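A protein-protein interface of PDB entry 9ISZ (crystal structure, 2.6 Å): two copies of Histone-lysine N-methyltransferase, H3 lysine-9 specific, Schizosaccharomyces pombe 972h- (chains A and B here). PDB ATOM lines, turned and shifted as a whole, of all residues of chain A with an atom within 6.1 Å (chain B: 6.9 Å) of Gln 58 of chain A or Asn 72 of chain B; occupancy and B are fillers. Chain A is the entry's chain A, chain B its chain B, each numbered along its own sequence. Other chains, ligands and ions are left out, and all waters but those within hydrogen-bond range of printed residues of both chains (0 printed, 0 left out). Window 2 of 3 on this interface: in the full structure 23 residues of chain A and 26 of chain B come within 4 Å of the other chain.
O of Ser 120 of chain B lies close to O of Thr 57 of chain A (3.5 Å). O of Phe 121 of chain B is in hydrogen-bond range of NE2 of Gln 58 of chain A, 3.1 Å away. The side-chain amide nitrogen (NE2) of Gln 58 of chain A is in hydrogen-bond range of the side-chain amide oxygen (OD1) of Asn 72 of chain B (3.3 Å).
Ser 120 of chain B touches Leu 56 of chain A (OG to CB, 3.2 Å). Gln 58 of chain A touches Cys 71 of chain B (NE2 to O, 3.9 Å). Gln 58 of chain A touches Ser 120 of chain B. CG of Gln 58 of chain A touches O of Cys 122 of chain B, 3.2 Å away. Ser 123 of chain B touches Gln 58 of chain A (CB to NE2, 3.5 Å). Phe 121 of chain B touches Val 60 of chain A (CE1 to O, 3.9 Å).
Of the 8 printed residues of chain A, 4 touch a printed residue of chain B. Hydrophobic or aromatic side chains of chain A within 4 Å of the printed part of chain B: Leu 56. Of the 17 printed residues of chain B, 6 touch a printed residue of chain A. Along chain B the printed residues that touch a printed residue of chain A span positions 71 to 123. Among the printed residues, no Asp or Glu carboxylate lies within 4 Å of a Lys or Arg side-chain nitrogen of the other chain.
Printed residues of chain B within 4 Å of Leu 56 of chain A: Ser 120 (3.2 Å). Of the printed residues of chain B, Thr 57 of chain A touches Ser 120 (3.5 Å). Gln 58 of chain A touches six residues of chain B. Of chain A, only Gln 58 comes within 4 Å of Asn 72 of chain B. Cys 79 of chain B touches none of the printed residues of chain A. Glu 88 of chain B touches none of the printed residues of chain A. The nearest printed residue of chain A that does not touch Asn 72 of chain B is Gly 59 of chain A (8.8 Å). The nearest printed residue of chain A that does not touch Ser 123 of chain B is Thr 57 of chain A (7.3 Å).
No position is printed for both chains. Of the 9 pairs that touch across the chains among the printed residues, none has its exchanged pair printed and touching as well.
NH2 of Arg 86 of chain B is in hydrogen-bond range of O of Asn 72 of chain B (3.0 Å). The side-chain hydroxyl (OG) of Ser 74 of chain B sits at hydrogen-bond distance from the side-chain hydroxyl (OG) of Ser 123 of chain B (3.1 Å). O of Cys 71 of chain B sits at hydrogen-bond distance from N of Ser 123 of chain B (3.1 Å). O of Asn 72 of chain B is in hydrogen-bond range of OG of Ser 75 of chain B. N of Cys 73 of chain B sits at hydrogen-bond distance from OG of Ser 123 of chain B (3.5 Å). The side-chain carboxylate (OE1) of Glu 88 of chain B is in hydrogen-bond range of the backbone NH (N) of Asn 72 of chain B, at 3.1 Å.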
ATOM      1  N   LEU A  56     -34.514   4.621  -2.560  1.00  0.00           N
ATOM      2  CA  LEU A  56     -33.147   4.287  -2.926  1.00  0.00           C
ATOM      3  C   LEU A  56     -32.356   3.856  -1.696  1.00  0.00           C
ATOM      4  O   LEU A  56     -32.644   4.265  -0.568  1.00  0.00           O
ATOM      5  CB  LEU A  56     -32.472   5.482  -3.596  1.00  0.00           C
ATOM      6  CG  LEU A  56     -33.316   6.204  -4.646  1.00  0.00           C
ATOM      7  CD1 LEU A  56     -32.620   7.468  -5.114  1.00  0.00           C
ATOM      8  CD2 LEU A  56     -33.614   5.287  -5.818  1.00  0.00           C
ATOM      9  N   THR A  57     -31.351   3.016  -1.922  1.00  0.00           N
ATOM     10  CA  THR A  57     -30.515   2.473  -0.859  1.00  0.00           C
ATOM     11  C   THR A  57     -29.060   2.889  -1.080  1.00  0.00           C
ATOM     12  O   THR A  57     -28.742   3.666  -1.986  1.00  0.00           O
ATOM     13  CB  THR A  57     -30.661   0.950  -0.792  1.00  0.00           C
ATOM     14  OG1 THR A  57     -30.296   0.378  -2.055  1.00  0.00           O
ATOM     15  CG2 THR A  57     -32.096   0.570  -0.466  1.00  0.00           C
ATOM     16  N   GLN A  58     -28.174   2.366  -0.234  1.00  0.00           N
ATOM     17  CA  GLN A  58     -26.754   2.678  -0.338  1.00  0.00           C
ATOM     18  C   GLN A  58     -26.164   2.101  -1.619  1.00  0.00           C
ATOM     19  O   GLN A  58     -26.479   0.976  -2.017  1.00  0.00           O
ATOM     20  CB  GLN A  58     -25.994   2.129   0.868  1.00  0.00           C
ATOM     21  CG  GLN A  58     -25.730   3.147   1.960  1.00  0.00           C
ATOM     22  CD  GLN A  58     -24.522   2.788   2.814  1.00  0.00           C
ATOM     23  OE1 GLN A  58     -24.100   1.632   2.861  1.00  0.00           O
ATOM     24  NE2 GLN A  58     -23.957   3.786   3.488  1.00  0.00           N
ATOM     25  N   GLY A  59     -25.289   2.875  -2.255  1.00  0.00           N
ATOM     26  CA  GLY A  59     -24.639   2.420  -3.466  1.00  0.00           C
ATOM     27  C   GLY A  59     -25.491   2.482  -4.710  1.00  0.00           C
ATOM     28  O   GLY A  59     -25.156   1.838  -5.708  1.00  0.00           O
ATOM     29  N   VAL A  60     -26.588   3.232  -4.683  1.00  0.00           N
ATOM     30  CA  VAL A  60     -27.468   3.395  -5.832  1.00  0.00           C
ATOM     31  C   VAL A  60     -27.360   4.851  -6.265  1.00  0.00           C
ATOM     32  O   VAL A  60     -27.916   5.744  -5.614  1.00  0.00           O
ATOM     33  CB  VAL A  60     -28.915   3.011  -5.510  1.00  0.00           C
ATOM     34  CG1 VAL A  60     -29.807   3.247  -6.720  1.00  0.00           C
ATOM     35  CG2 VAL A  60     -28.991   1.561  -5.056  1.00  0.00           C
ATOM     36  N   VAL A 172     -34.905   0.379  -4.157  1.00  0.00           N
ATOM     37  CA  VAL A 172     -33.951   0.274  -5.256  1.00  0.00           C
ATOM     38  C   VAL A 172     -32.608  -0.135  -4.668  1.00  0.00           C
ATOM     39  O   VAL A 172     -32.058   0.560  -3.808  1.00  0.00           O
ATOM     40  CB  VAL A 172     -33.842   1.592  -6.036  1.00  0.00           C
ATOM     41  CG1 VAL A 172     -32.994   1.392  -7.282  1.00  0.00           C
ATOM     42  CG2 VAL A 172     -35.223   2.098  -6.407  1.00  0.00           C
ATOM     43  N   ILE A 173     -32.085  -1.276  -5.119  1.00  0.00           N
ATOM     44  CA  ILE A 173     -30.873  -1.859  -4.566  1.00  0.00           C
ATOM     45  C   ILE A 173     -29.921  -2.205  -5.701  1.00  0.00           C
ATOM     46  O   ILE A 173     -30.319  -2.389  -6.856  1.00  0.00           O
ATOM     47  CB  ILE A 173     -31.166  -3.111  -3.708  1.00  0.00           C
ATOM     48  CG1 ILE A 173     -31.824  -4.203  -4.555  1.00  0.00           C
ATOM     49  CG2 ILE A 173     -32.036  -2.753  -2.510  1.00  0.00           C
ATOM     50  CD1 ILE A 173     -32.279  -5.407  -3.758  1.00  0.00           C
ATOM     51  N   THR A 174     -28.642  -2.293  -5.347  1.00  0.00           N
ATOM     52  CA  THR A 174     -27.605  -2.589  -6.319  1.00  0.00           C
ATOM     53  C   THR A 174     -27.633  -4.068  -6.692  1.00  0.00           C
ATOM     54  O   THR A 174     -28.354  -4.877  -6.104  1.00  0.00           O
ATOM     55  CB  THR A 174     -26.233  -2.207  -5.770  1.00  0.00           C
ATOM     56  OG1 THR A 174     -25.218  -2.616  -6.697  1.00  0.00           O
ATOM     57  CG2 THR A 174     -25.989  -2.882  -4.430  1.00  0.00           C
ATOM     58  N   GLY B  70     -24.214  10.309   2.909  1.00  0.00           N
ATOM     59  CA  GLY B  70     -24.894   9.556   3.938  1.00  0.00           C
ATOM     60  C   GLY B  70     -23.997   9.264   5.128  1.00  0.00           C
ATOM     61  O   GLY B  70     -22.821   9.621   5.170  1.00  0.00           O
ATOM     62  N   CYS B  71     -24.580   8.597   6.116  1.00  0.00           N
ATOM     63  CA  CYS B  71     -23.872   8.199   7.319  1.00  0.00           C
ATOM     64  C   CYS B  71     -23.758   6.680   7.372  1.00  0.00           C
ATOM     65  O   CYS B  71     -24.452   5.956   6.652  1.00  0.00           O
ATOM     66  CB  CYS B  71     -24.578   8.726   8.572  1.00  0.00           C
ATOM     67  SG  CYS B  71     -26.118   7.878   8.968  1.00  0.00           S
ATOM     68  N   ASN B  72     -22.861   6.200   8.233  1.00  0.00           N
ATOM     69  CA  ASN B  72     -22.596   4.771   8.327  1.00  0.00           C
ATOM     70  C   ASN B  72     -22.891   4.244   9.726  1.00  0.00           C
ATOM     71  O   ASN B  72     -22.103   3.478  10.294  1.00  0.00           O
ATOM     72  CB  ASN B  72     -21.153   4.466   7.916  1.00  0.00           C
ATOM     73  CG  ASN B  72     -20.882   4.802   6.460  1.00  0.00           C
ATOM     74  OD1 ASN B  72     -21.351   4.111   5.554  1.00  0.00           O
ATOM     75  ND2 ASN B  72     -20.120   5.867   6.226  1.00  0.00           N
ATOM     76  N   CYS B  73     -24.030   4.648  10.284  1.00  0.00           N
ATOM     77  CA  CYS B  73     -24.411   4.260  11.635  1.00  0.00           C
ATOM     78  C   CYS B  73     -25.029   2.872  11.723  1.00  0.00           C
ATOM     79  O   CYS B  73     -25.403   2.452  12.824  1.00  0.00           O
ATOM     80  CB  CYS B  73     -25.383   5.288  12.212  1.00  0.00           C
ATOM     81  SG  CYS B  73     -24.669   6.924  12.419  1.00  0.00           S
ATOM     82  N   SER B  74     -25.155   2.158  10.602  1.00  0.00           N
ATOM     83  CA  SER B  74     -25.668   0.793  10.658  1.00  0.00           C
ATOM     84  C   SER B  74     -24.797  -0.091  11.537  1.00  0.00           C
ATOM     85  O   SER B  74     -25.295  -1.049  12.139  1.00  0.00           O
ATOM     86  CB  SER B  74     -25.763   0.205   9.251  1.00  0.00           C
ATOM     87  OG  SER B  74     -24.476   0.052   8.677  1.00  0.00           O
ATOM     88  N   SER B  75     -23.499   0.212  11.626  1.00  0.00           N
ATOM     89  CA  SER B  75     -22.619  -0.557  12.499  1.00  0.00           C
ATOM     90  C   SER B  75     -22.904  -0.278  13.970  1.00  0.00           C
ATOM     91  O   SER B  75     -22.654  -1.138  14.822  1.00  0.00           O
ATOM     92  CB  SER B  75     -21.156  -0.263  12.162  1.00  0.00           C
ATOM     93  OG  SER B  75     -20.824   1.087  12.428  1.00  0.00           O
ATOM     94  N   LEU B  76     -23.428   0.907  14.291  1.00  0.00           N
ATOM     95  CA  LEU B  76     -23.867   1.194  15.651  1.00  0.00           C
ATOM     96  C   LEU B  76     -25.187   0.521  15.998  1.00  0.00           C
ATOM     97  O   LEU B  76     -25.535   0.443  17.183  1.00  0.00           O
ATOM     98  CB  LEU B  76     -24.015   2.702  15.863  1.00  0.00           C
ATOM     99  CG  LEU B  76     -22.792   3.610  15.703  1.00  0.00           C
ATOM    100  CD1 LEU B  76     -23.157   5.028  16.119  1.00  0.00           C
ATOM    101  CD2 LEU B  76     -21.616   3.096  16.507  1.00  0.00           C
ATOM    102  N   CYS B  79     -28.214   4.333  13.806  1.00  0.00           N
ATOM    103  CA  CYS B  79     -28.269   5.748  14.181  1.00  0.00           C
ATOM    104  C   CYS B  79     -28.733   5.933  15.632  1.00  0.00           C
ATOM    105  O   CYS B  79     -29.830   6.417  15.907  1.00  0.00           O
ATOM    106  CB  CYS B  79     -29.169   6.543  13.223  1.00  0.00           C
ATOM    107  SG  CYS B  79     -28.425   6.999  11.623  1.00  0.00           S
ATOM    108  N   ARG B  86     -21.229  10.291  16.349  1.00  0.00           N
ATOM    109  CA  ARG B  86     -20.816   9.288  15.377  1.00  0.00           C
ATOM    110  C   ARG B  86     -21.579   9.382  14.062  1.00  0.00           C
ATOM    111  O   ARG B  86     -21.217   8.691  13.103  1.00  0.00           O
ATOM    112  CB  ARG B  86     -20.989   7.887  15.968  1.00  0.00           C
ATOM    113  CG  ARG B  86     -19.684   7.140  16.196  1.00  0.00           C
ATOM    114  CD  ARG B  86     -18.942   6.933  14.886  1.00  0.00           C
ATOM    115  NE  ARG B  86     -19.777   6.284  13.882  1.00  0.00           N
ATOM    116  CZ  ARG B  86     -19.842   4.973  13.695  1.00  0.00           C
ATOM    117  NH1 ARG B  86     -19.130   4.132  14.431  1.00  0.00           N
ATOM    118  NH2 ARG B  86     -20.644   4.492  12.749  1.00  0.00           N
ATOM    119  N   CYS B  87     -22.615  10.213  13.992  1.00  0.00           N
ATOM    120  CA  CYS B  87     -23.432  10.337  12.793  1.00  0.00           C
ATOM    121  C   CYS B  87     -22.841  11.404  11.877  1.00  0.00           C
ATOM    122  O   CYS B  87     -22.601  12.538  12.309  1.00  0.00           O
ATOM    123  CB  CYS B  87     -24.874  10.688  13.170  1.00  0.00           C
ATOM    124  SG  CYS B  87     -26.139  10.255  11.947  1.00  0.00           S
ATOM    125  N   GLU B  88     -22.599  11.037  10.615  1.00  0.00           N
ATOM    126  CA  GLU B  88     -22.080  12.009   9.657  1.00  0.00           C
ATOM    127  C   GLU B  88     -23.100  13.098   9.348  1.00  0.00           C
ATOM    128  O   GLU B  88     -22.720  14.243   9.091  1.00  0.00           O
ATOM    129  CB  GLU B  88     -21.650  11.314   8.364  1.00  0.00           C
ATOM    130  CG  GLU B  88     -20.345  10.536   8.462  1.00  0.00           C
ATOM    131  CD  GLU B  88     -20.551   9.072   8.800  1.00  0.00           C
ATOM    132  OE1 GLU B  88     -21.532   8.747   9.503  1.00  0.00           O
ATOM    133  OE2 GLU B  88     -19.727   8.243   8.355  1.00  0.00           O
ATOM    134  N   CYS B  89     -24.392  12.770   9.394  1.00  0.00           N
ATOM    135  CA  CYS B  89     -25.432  13.737   9.063  1.00  0.00           C
ATOM    136  C   CYS B  89     -25.429  14.933  10.001  1.00  0.00           C
ATOM    137  O   CYS B  89     -26.024  15.967   9.675  1.00  0.00           O
ATOM    138  CB  CYS B  89     -26.799  13.068   9.101  1.00  0.00           C
ATOM    139  SG  CYS B  89     -26.929  11.620   8.052  1.00  0.00           S
ATOM    140  N   SER B 120     -30.976   8.962   1.298  1.00  0.00           N
ATOM    141  CA  SER B 120     -30.860   7.697   0.577  1.00  0.00           C
ATOM    142  C   SER B 120     -29.481   7.069   0.731  1.00  0.00           C
ATOM    143  O   SER B 120     -29.357   5.841   0.681  1.00  0.00           O
ATOM    144  CB  SER B 120     -31.176   7.914  -0.904  1.00  0.00           C
ATOM    145  OG  SER B 120     -30.444   7.026  -1.722  1.00  0.00           O
ATOM    146  N   PHE B 121     -28.439   7.885   0.908  1.00  0.00           N
ATOM    147  CA  PHE B 121     -27.070   7.384   0.959  1.00  0.00           C
ATOM    148  C   PHE B 121     -26.684   6.810   2.317  1.00  0.00           C
ATOM    149  O   PHE B 121     -25.592   6.250   2.440  1.00  0.00           O
ATOM    150  CB  PHE B 121     -26.084   8.496   0.584  1.00  0.00           C
ATOM    151  CG  PHE B 121     -26.180   8.937  -0.851  1.00  0.00           C
ATOM    152  CD1 PHE B 121     -26.839   8.159  -1.790  1.00  0.00           C
ATOM    153  CD2 PHE B 121     -25.599  10.126  -1.263  1.00  0.00           C
ATOM    154  CE1 PHE B 121     -26.923   8.562  -3.110  1.00  0.00           C
ATOM    155  CE2 PHE B 121     -25.680  10.534  -2.582  1.00  0.00           C
ATOM    156  CZ  PHE B 121     -26.342   9.751  -3.506  1.00  0.00           C
ATOM    157  N   CYS B 122     -27.533   6.941   3.331  1.00  0.00           N
ATOM    158  CA  CYS B 122     -27.217   6.406   4.644  1.00  0.00           C
ATOM    159  C   CYS B 122     -27.413   4.892   4.672  1.00  0.00           C
ATOM    160  O   CYS B 122     -28.079   4.308   3.813  1.00  0.00           O
ATOM    161  CB  CYS B 122     -28.079   7.071   5.717  1.00  0.00           C
ATOM    162  SG  CYS B 122     -27.827   8.852   5.850  1.00  0.00           S
ATOM    163  N   SER B 123     -26.819   4.255   5.680  1.00  0.00           N
ATOM    164  CA  SER B 123     -26.876   2.806   5.836  1.00  0.00           C
ATOM    165  C   SER B 123     -27.949   2.361   6.822  1.00  0.00           C
ATOM    166  O   SER B 123     -27.990   1.182   7.188  1.00  0.00           O
ATOM    167  CB  SER B 123     -25.510   2.264   6.271  1.00  0.00           C
ATOM    168  OG  SER B 123     -25.091   2.844   7.493  1.00  0.00           O
ATOM    169  N   CYS B 124     -28.810   3.273   7.263  1.00  0.00           N
ATOM    170  CA  CYS B 124     -29.860   2.942   8.208  1.00  0.00           C
ATOM    171  C   CYS B 124     -31.158   2.622   7.468  1.00  0.00           C
ATOM    172  O   CYS B 124     -31.247   2.718   6.241  1.00  0.00           O
ATOM    173  CB  CYS B 124     -30.051   4.087   9.197  1.00  0.00           C
ATOM    174  SG  CYS B 124     -30.285   5.680   8.394  1.00  0.00           S
